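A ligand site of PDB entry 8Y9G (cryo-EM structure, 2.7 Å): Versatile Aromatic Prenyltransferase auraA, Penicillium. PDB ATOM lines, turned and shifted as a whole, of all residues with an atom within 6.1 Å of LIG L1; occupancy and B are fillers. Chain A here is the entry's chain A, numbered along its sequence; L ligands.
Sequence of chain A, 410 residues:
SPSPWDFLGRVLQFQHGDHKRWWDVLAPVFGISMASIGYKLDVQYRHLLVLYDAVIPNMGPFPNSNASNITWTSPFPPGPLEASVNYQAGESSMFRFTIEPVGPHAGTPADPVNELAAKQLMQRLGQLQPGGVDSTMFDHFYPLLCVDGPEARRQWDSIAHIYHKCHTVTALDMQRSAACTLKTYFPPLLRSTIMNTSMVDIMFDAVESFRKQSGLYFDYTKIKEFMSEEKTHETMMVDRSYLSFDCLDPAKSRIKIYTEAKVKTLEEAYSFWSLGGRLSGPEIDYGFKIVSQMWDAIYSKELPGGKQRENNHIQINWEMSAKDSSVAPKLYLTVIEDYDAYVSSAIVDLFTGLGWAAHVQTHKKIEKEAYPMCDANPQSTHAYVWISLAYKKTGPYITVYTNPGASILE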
ATOM      1  N   PHE A  76      12.193  22.916  19.827  1.00  0.00           N
ATOM      2  CA  PHE A  76      12.136  23.557  21.123  1.00  0.00           C
ATOM      3  C   PHE A  76      11.438  24.913  21.008  1.00  0.00           C
ATOM      4  O   PHE A  76      11.563  25.594  19.985  1.00  0.00           O
ATOM      5  CB  PHE A  76      13.531  23.753  21.690  1.00  0.00           C
ATOM      6  CG  PHE A  76      14.437  22.572  21.514  1.00  0.00           C
ATOM      7  CD1 PHE A  76      15.207  22.427  20.378  1.00  0.00           C
ATOM      8  CD2 PHE A  76      14.519  21.609  22.495  1.00  0.00           C
ATOM      9  CE1 PHE A  76      16.026  21.351  20.225  1.00  0.00           C
ATOM     10  CE2 PHE A  76      15.345  20.521  22.347  1.00  0.00           C
ATOM     11  CZ  PHE A  76      16.103  20.395  21.211  1.00  0.00           C
ATOM     12  N   LEU A  81      17.051  26.712  25.737  1.00  0.00           N
ATOM     13  CA  LEU A  81      16.624  25.327  25.767  1.00  0.00           C
ATOM     14  C   LEU A  81      16.424  24.851  27.187  1.00  0.00           C
ATOM     15  O   LEU A  81      15.698  23.870  27.425  1.00  0.00           O
ATOM     16  CB  LEU A  81      17.660  24.452  25.062  1.00  0.00           C
ATOM     17  CG  LEU A  81      18.148  24.921  23.700  1.00  0.00           C
ATOM     18  CD1 LEU A  81      19.209  23.982  23.197  1.00  0.00           C
ATOM     19  CD2 LEU A  81      17.006  25.012  22.718  1.00  0.00           C
ATOM     20  N   GLU A  82      17.094  25.488  28.112  1.00  0.00           N
ATOM     21  CA  GLU A  82      16.978  25.159  29.478  1.00  0.00           C
ATOM     22  C   GLU A  82      17.575  26.161  30.394  1.00  0.00           C
ATOM     23  O   GLU A  82      18.280  26.988  29.932  1.00  0.00           O
ATOM     24  CB  GLU A  82      17.670  23.842  29.767  1.00  0.00           C
ATOM     25  CG  GLU A  82      19.119  23.767  29.335  1.00  0.00           C
ATOM     26  CD  GLU A  82      20.182  24.004  30.407  1.00  0.00           C
ATOM     27  OE1 GLU A  82      21.158  23.276  30.417  1.00  0.00           O
ATOM     28  OE2 GLU A  82      20.177  24.946  31.195  1.00  0.00           O
ATOM     29  N   THR A  98      21.410  26.997  29.074  1.00  0.00           N
ATOM     30  CA  THR A  98      21.805  26.663  27.726  1.00  0.00           C
ATOM     31  C   THR A  98      21.003  27.498  26.746  1.00  0.00           C
ATOM     32  O   THR A  98      19.821  27.774  26.970  1.00  0.00           O
ATOM     33  CB  THR A  98      21.590  25.176  27.406  1.00  0.00           C
ATOM     34  OG1 THR A  98      22.252  24.375  28.385  1.00  0.00           O
ATOM     35  CG2 THR A  98      22.154  24.852  26.034  1.00  0.00           C
ATOM     36  N   GLU A 100      20.627  27.978  22.318  1.00  0.00           N
ATOM     37  CA  GLU A 100      21.022  27.833  20.935  1.00  0.00           C
ATOM     38  C   GLU A 100      21.129  29.222  20.329  1.00  0.00           C
ATOM     39  O   GLU A 100      20.088  29.848  20.094  1.00  0.00           O
ATOM     40  CB  GLU A 100      20.014  26.993  20.172  1.00  0.00           C
ATOM     41  CG  GLU A 100      20.389  26.742  18.728  1.00  0.00           C
ATOM     42  CD  GLU A 100      19.182  26.468  17.862  1.00  0.00           C
ATOM     43  OE1 GLU A 100      18.185  25.928  18.382  1.00  0.00           O
ATOM     44  OE2 GLU A 100      19.231  26.803  16.664  1.00  0.00           O
ATOM     45  N   HIS A 164      15.372  21.194  11.938  1.00  0.00           N
ATOM     46  CA  HIS A 164      16.203  21.951  12.865  1.00  0.00           C
ATOM     47  C   HIS A 164      17.619  21.961  12.320  1.00  0.00           C
ATOM     48  O   HIS A 164      18.390  21.028  12.541  1.00  0.00           O
ATOM     49  CB  HIS A 164      16.143  21.362  14.265  1.00  0.00           C
ATOM     50  CG  HIS A 164      16.635  22.278  15.334  1.00  0.00           C
ATOM     51  ND1 HIS A 164      16.923  21.840  16.604  1.00  0.00           N
ATOM     52  CD2 HIS A 164      16.883  23.612  15.324  1.00  0.00           C
ATOM     53  CE1 HIS A 164      17.334  22.865  17.337  1.00  0.00           C
ATOM     54  NE2 HIS A 164      17.316  23.951  16.588  1.00  0.00           N
ATOM     55  N   CYS A 166      20.340  23.061  13.213  1.00  0.00           N
ATOM     56  CA  CYS A 166      21.219  23.443  14.298  1.00  0.00           C
ATOM     57  C   CYS A 166      22.620  22.887  14.063  1.00  0.00           C
ATOM     58  O   CYS A 166      22.781  21.753  13.609  1.00  0.00           O
ATOM     59  CB  CYS A 166      20.673  22.933  15.626  1.00  0.00           C
ATOM     60  SG  CYS A 166      21.763  23.073  17.053  1.00  0.00           S
ATOM     61  N   THR A 168      25.516  24.519  16.275  1.00  0.00           N
ATOM     62  CA  THR A 168      26.298  24.820  17.467  1.00  0.00           C
ATOM     63  C   THR A 168      25.373  25.385  18.528  1.00  0.00           C
ATOM     64  O   THR A 168      24.591  26.296  18.267  1.00  0.00           O
ATOM     65  CB  THR A 168      27.441  25.807  17.176  1.00  0.00           C
ATOM     66  OG1 THR A 168      28.143  26.086  18.393  1.00  0.00           O
ATOM     67  CG2 THR A 168      26.924  27.085  16.596  1.00  0.00           C
ATOM     68  N   VAL A 169      25.473  24.827  19.725  1.00  0.00           N
ATOM     69  CA  VAL A 169      24.697  25.252  20.887  1.00  0.00           C
ATOM     70  C   VAL A 169      25.668  25.659  21.977  1.00  0.00           C
ATOM     71  O   VAL A 169      26.724  25.022  22.158  1.00  0.00           O
ATOM     72  CB  VAL A 169      23.751  24.130  21.367  1.00  0.00           C
ATOM     73  CG1 VAL A 169      23.304  24.363  22.790  1.00  0.00           C
ATOM     74  CG2 VAL A 169      22.579  24.024  20.447  1.00  0.00           C
ATOM     75  N   ALA A 171      26.187  26.680  26.046  1.00  0.00           N
ATOM     76  CA  ALA A 171      25.758  26.709  27.437  1.00  0.00           C
ATOM     77  C   ALA A 171      26.733  27.529  28.246  1.00  0.00           C
ATOM     78  O   ALA A 171      27.945  27.471  28.013  1.00  0.00           O
ATOM     79  CB  ALA A 171      25.653  25.295  28.021  1.00  0.00           C
ATOM     80  N   TYR A 185      28.200  22.795  22.171  1.00  0.00           N
ATOM     81  CA  TYR A 185      27.661  21.520  21.719  1.00  0.00           C
ATOM     82  C   TYR A 185      27.567  21.568  20.200  1.00  0.00           C
ATOM     83  O   TYR A 185      26.993  22.501  19.641  1.00  0.00           O
ATOM     84  CB  TYR A 185      26.277  21.251  22.317  1.00  0.00           C
ATOM     85  CG  TYR A 185      26.194  21.357  23.817  1.00  0.00           C
ATOM     86  CD1 TYR A 185      26.235  22.574  24.447  1.00  0.00           C
ATOM     87  CD2 TYR A 185      26.040  20.228  24.599  1.00  0.00           C
ATOM     88  CE1 TYR A 185      26.148  22.677  25.812  1.00  0.00           C
ATOM     89  CE2 TYR A 185      25.948  20.317  25.961  1.00  0.00           C
ATOM     90  CZ  TYR A 185      26.006  21.545  26.567  1.00  0.00           C
ATOM     91  OH  TYR A 185      25.921  21.643  27.919  1.00  0.00           O
ATOM     92  N   PHE A 186      28.132  20.566  19.547  1.00  0.00           N
ATOM     93  CA  PHE A 186      28.106  20.488  18.091  1.00  0.00           C
ATOM     94  C   PHE A 186      27.264  19.304  17.642  1.00  0.00           C
ATOM     95  O   PHE A 186      27.728  18.156  17.743  1.00  0.00           O
ATOM     96  CB  PHE A 186      29.525  20.358  17.543  1.00  0.00           C
ATOM     97  CG  PHE A 186      30.260  21.660  17.456  1.00  0.00           C
ATOM     98  CD1 PHE A 186      29.761  22.708  16.710  1.00  0.00           C
ATOM     99  CD2 PHE A 186      31.469  21.820  18.096  1.00  0.00           C
ATOM    100  CE1 PHE A 186      30.437  23.895  16.626  1.00  0.00           C
ATOM    101  CE2 PHE A 186      32.154  23.013  18.013  1.00  0.00           C
ATOM    102  CZ  PHE A 186      31.635  24.054  17.280  1.00  0.00           C
ATOM    103  N   PRO A 187      26.043  19.520  17.170  1.00  0.00           N
ATOM    104  CA  PRO A 187      25.345  18.466  16.441  1.00  0.00           C
ATOM    105  C   PRO A 187      25.767  18.443  14.988  1.00  0.00           C
ATOM    106  O   PRO A 187      25.432  19.355  14.216  1.00  0.00           O
ATOM    107  CB  PRO A 187      23.873  18.863  16.587  1.00  0.00           C
ATOM    108  CG  PRO A 187      23.895  20.310  16.756  1.00  0.00           C
ATOM    109  CD  PRO A 187      25.147  20.638  17.508  1.00  0.00           C
ATOM    110  N   ARG A 240      20.261  12.229  16.114  1.00  0.00           N
ATOM    111  CA  ARG A 240      20.063  13.235  17.153  1.00  0.00           C
ATOM    112  C   ARG A 240      21.252  13.351  18.094  1.00  0.00           C
ATOM    113  O   ARG A 240      21.117  13.913  19.180  1.00  0.00           O
ATOM    114  CB  ARG A 240      18.802  12.895  17.955  1.00  0.00           C
ATOM    115  CG  ARG A 240      17.564  12.597  17.122  1.00  0.00           C
ATOM    116  CD  ARG A 240      16.682  13.813  16.992  1.00  0.00           C
ATOM    117  NE  ARG A 240      17.338  14.894  16.267  1.00  0.00           N
ATOM    118  CZ  ARG A 240      17.370  14.998  14.935  1.00  0.00           C
ATOM    119  NH1 ARG A 240      16.792  14.071  14.178  1.00  0.00           N
ATOM    120  NH2 ARG A 240      17.990  16.015  14.374  1.00  0.00           N
ATOM    121  N   TYR A 242      25.216  14.422  19.339  1.00  0.00           N
ATOM    122  CA  TYR A 242      26.003  15.641  19.270  1.00  0.00           C
ATOM    123  C   TYR A 242      27.170  15.528  20.247  1.00  0.00           C
ATOM    124  O   TYR A 242      27.148  14.732  21.194  1.00  0.00           O
ATOM    125  CB  TYR A 242      25.142  16.870  19.565  1.00  0.00           C
ATOM    126  CG  TYR A 242      24.447  16.851  20.902  1.00  0.00           C
ATOM    127  CD1 TYR A 242      23.269  16.143  21.082  1.00  0.00           C
ATOM    128  CD2 TYR A 242      24.942  17.554  21.984  1.00  0.00           C
ATOM    129  CE1 TYR A 242      22.629  16.122  22.301  1.00  0.00           C
ATOM    130  CE2 TYR A 242      24.303  17.549  23.199  1.00  0.00           C
ATOM    131  CZ  TYR A 242      23.142  16.830  23.346  1.00  0.00           C
ATOM    132  OH  TYR A 242      22.510  16.814  24.565  1.00  0.00           O
ATOM    133  N   TYR A 258      26.872  12.829  23.117  1.00  0.00           N
ATOM    134  CA  TYR A 258      25.467  12.711  23.458  1.00  0.00           C
ATOM    135  C   TYR A 258      24.717  11.946  22.381  1.00  0.00           C
ATOM    136  O   TYR A 258      25.126  11.946  21.209  1.00  0.00           O
ATOM    137  CB  TYR A 258      24.826  14.091  23.627  1.00  0.00           C
ATOM    138  CG  TYR A 258      25.363  14.919  24.758  1.00  0.00           C
ATOM    139  CD1 TYR A 258      26.530  15.647  24.601  1.00  0.00           C
ATOM    140  CD2 TYR A 258      24.693  15.021  25.959  1.00  0.00           C
ATOM    141  CE1 TYR A 258      27.016  16.417  25.624  1.00  0.00           C
ATOM    142  CE2 TYR A 258      25.172  15.803  26.976  1.00  0.00           C
ATOM    143  CZ  TYR A 258      26.335  16.497  26.807  1.00  0.00           C
ATOM    144  OH  TYR A 258      26.817  17.276  27.834  1.00  0.00           O
ATOM    145  N   GLU A 260      20.346  10.404  21.578  1.00  0.00           N
ATOM    146  CA  GLU A 260      18.951  10.255  21.982  1.00  0.00           C
ATOM    147  C   GLU A 260      18.502   8.813  21.794  1.00  0.00           C
ATOM    148  O   GLU A 260      18.882   8.166  20.814  1.00  0.00           O
ATOM    149  CB  GLU A 260      18.037  11.190  21.187  1.00  0.00           C
ATOM    150  CG  GLU A 260      18.384  12.658  21.293  1.00  0.00           C
ATOM    151  CD  GLU A 260      17.235  13.568  20.949  1.00  0.00           C
ATOM    152  OE1 GLU A 260      16.085  13.082  20.864  1.00  0.00           O
ATOM    153  OE2 GLU A 260      17.471  14.774  20.745  1.00  0.00           O
ATOM    154  N   GLN A 315      18.010  10.897  26.850  1.00  0.00           N
ATOM    155  CA  GLN A 315      19.301  11.203  26.272  1.00  0.00           C
ATOM    156  C   GLN A 315      20.386  10.688  27.210  1.00  0.00           C
ATOM    157  O   GLN A 315      20.133  10.338  28.361  1.00  0.00           O
ATOM    158  CB  GLN A 315      19.479  12.714  26.042  1.00  0.00           C
ATOM    159  CG  GLN A 315      18.332  13.384  25.331  1.00  0.00           C
ATOM    160  CD  GLN A 315      18.754  14.678  24.672  1.00  0.00           C
ATOM    161  OE1 GLN A 315      19.939  14.934  24.474  1.00  0.00           O
ATOM    162  NE2 GLN A 315      17.774  15.504  24.333  1.00  0.00           N
ATOM    163  N   TRP A 386      13.951  18.252  31.655  1.00  0.00           N
ATOM    164  CA  TRP A 386      14.946  17.195  31.760  1.00  0.00           C
ATOM    165  C   TRP A 386      15.347  17.005  33.210  1.00  0.00           C
ATOM    166  O   TRP A 386      15.310  17.942  34.017  1.00  0.00           O
ATOM    167  CB  TRP A 386      16.216  17.498  30.941  1.00  0.00           C
ATOM    168  CG  TRP A 386      16.087  17.283  29.481  1.00  0.00           C
ATOM    169  CD1 TRP A 386      15.889  16.091  28.851  1.00  0.00           C
ATOM    170  CD2 TRP A 386      16.162  18.275  28.454  1.00  0.00           C
ATOM    171  NE1 TRP A 386      15.829  16.286  27.494  1.00  0.00           N
ATOM    172  CE2 TRP A 386      15.989  17.613  27.227  1.00  0.00           C
ATOM    173  CE3 TRP A 386      16.348  19.654  28.458  1.00  0.00           C
ATOM    174  CZ2 TRP A 386      16.015  18.290  26.019  1.00  0.00           C
ATOM    175  CZ3 TRP A 386      16.359  20.318  27.260  1.00  0.00           C
ATOM    176  CH2 TRP A 386      16.194  19.645  26.060  1.00  0.00           C
ATOM    177  N   TYR A 401      16.533  20.562  34.906  1.00  0.00           N
ATOM    178  CA  TYR A 401      16.352  21.549  33.851  1.00  0.00           C
ATOM    179  C   TYR A 401      14.920  22.044  33.868  1.00  0.00           C
ATOM    180  O   TYR A 401      13.995  21.318  34.224  1.00  0.00           O
ATOM    181  CB  TYR A 401      16.675  20.966  32.478  1.00  0.00           C
ATOM    182  CG  TYR A 401      18.087  20.475  32.345  1.00  0.00           C
ATOM    183  CD1 TYR A 401      18.520  19.359  33.028  1.00  0.00           C
ATOM    184  CD2 TYR A 401      18.992  21.126  31.540  1.00  0.00           C
ATOM    185  CE1 TYR A 401      19.787  18.915  32.912  1.00  0.00           C
ATOM    186  CE2 TYR A 401      20.289  20.689  31.418  1.00  0.00           C
ATOM    187  CZ  TYR A 401      20.674  19.576  32.116  1.00  0.00           C
ATOM    188  OH  TYR A 401      21.963  19.114  32.009  1.00  0.00           O
HETATM  189  C1  LIG L   1      20.868  20.597  25.437  1.00  0.00           C
HETATM  190  C2  LIG L   1      20.103  20.085  24.356  1.00  0.00           C
HETATM  191  C3  LIG L   1      20.559  19.568  23.183  1.00  0.00           C
HETATM  192  C4  LIG L   1      19.789  18.539  22.497  1.00  0.00           C
HETATM  193  N1  LIG L   1      20.146  18.329  21.232  1.00  0.00           N
HETATM  194  C5  LIG L   1      20.851  19.282  20.374  1.00  0.00           C
HETATM  195  C6  LIG L   1      21.912  19.965  21.214  1.00  0.00           C
HETATM  196  N2  LIG L   1      21.705  20.011  22.558  1.00  0.00           N
HETATM  197  O1  LIG L   1      18.878  17.936  23.033  1.00  0.00           O
HETATM  198  O2  LIG L   1      22.945  20.390  20.727  1.00  0.00           O
HETATM  199  C7  LIG L   1      20.509  20.869  26.727  1.00  0.00           C
HETATM  200  N3  LIG L   1      21.628  21.326  27.346  1.00  0.00           N
HETATM  201  C8  LIG L   1      22.617  21.319  26.461  1.00  0.00           C
HETATM  202  N4  LIG L   1      22.221  20.888  25.282  1.00  0.00           N
HETATM  203  C9  LIG L   1      19.861  20.212  19.644  1.00  0.00           C
HETATM  204  C10 LIG L   1      20.192  20.317  18.169  1.00  0.00           C
HETATM  205  C11 LIG L   1      19.702  21.584  20.273  1.00  0.00           C
HETATM  206  O1  LG2 L   2      26.400  19.190  33.302  1.00  0.00           O
HETATM  207  P1  LG2 L   2      27.370  19.026  32.201  1.00  0.00           P
HETATM  208  O2  LG2 L   2      28.357  20.131  32.150  1.00  0.00           O
HETATM  209  O3  LG2 L   2      27.958  17.660  32.087  1.00  0.00           O
HETATM  210  O4  LG2 L   2      26.614  19.244  30.833  1.00  0.00           O
HETATM  211  P2  LG2 L   2      25.053  19.250  30.666  1.00  0.00           P
HETATM  212  O5  LG2 L   2      24.460  20.644  31.084  1.00  0.00           O
HETATM  213  O6  LG2 L   2      24.527  18.113  31.420  1.00  0.00           O
HETATM  214  S1  LG2 L   2      24.308  19.187  28.811  1.00  0.00           S
HETATM  215  C1  LG2 L   2      22.840  18.212  28.799  1.00  0.00           C
HETATM  216  C2  LG2 L   2      22.030  18.470  27.552  1.00  0.00           C
HETATM  217  C3  LG2 L   2      20.553  18.333  27.851  1.00  0.00           C
HETATM  218  C4  LG2 L   2      19.873  17.549  26.768  1.00  0.00           C
HETATM  219  C5  LG2 L   2      20.331  17.598  29.138  1.00  0.00           C
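The side-chain hydroxyl (OH) of Tyr 185 lies close to a sulfur (S1) of LG2 L2 (3.1 Å).
OH of Tyr 258 sits close to S1 of LG2 L2, at 3.3 Å.
OH of Tyr 401 lies within hydrogen-bond range of O6 of LG2 L2.
OG1 of Thr 98 lies within hydrogen-bond range of N3 of LIG L1 (3.3 Å).
The side-chain amide nitrogen of Gln 315 lies within hydrogen-bond range of an oxygen (O1) of LIG L1.
N of Tyr 185 sits at hydrogen-bond distance from O of Val 169 (2.7 Å).
The backbone NH (N) of Tyr 258 is in hydrogen-bond range of the backbone carbonyl oxygen (O) of Tyr 242 (2.7 Å).
The side-chain hydroxyl (OH) of Tyr 242 lies within hydrogen-bond range of the side-chain amide oxygen (OE1) of Gln 315.
A ring nitrogen (NE2) of His 164 lies within hydrogen-bond range of the side-chain carboxylate of Glu 100 (2.8 Å).
N of Leu 81 lies within hydrogen-bond range of O of Thr 98 (3.2 Å).
The side-chain hydroxyl (OG1) of Thr 98 is in hydrogen-bond range of the side-chain carboxylate (OE1) of Glu 82 (2.6 Å).
Phe 76 touches LIG L1.
Leu 81 touches LIG L1 (CD1 to C11, 3.8 Å).
Glu 82 touches LIG L1.
His 164 touches LIG L1 (CE1 to C10, 3.9 Å).
Cys 166 touches LIG L1.
Val 169 touches LIG L1.
Tyr 185 touches LIG L1 (CZ to C8, 3.4 Å).
Pro 187 touches LIG L1.
Tyr 242 touches LIG L1 (CE1 to N1, 3.5 Å).
Hydrophobic or aromatic side chains that line LIG L1: Phe 76, Leu 81, His 164, Val 169, Tyr 185, Pro 187 and Tyr 242.
Along chain A the residues within 4 Å of LIG L1 span positions 76 to 315.
The nearest printed residue that does not touch LIG L1 is Glu 260 (4.1 Å).
A nitrogen (N3) of LIG L1 sits close to a sulfur (S1) of LG2 L2 (3.7 Å).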
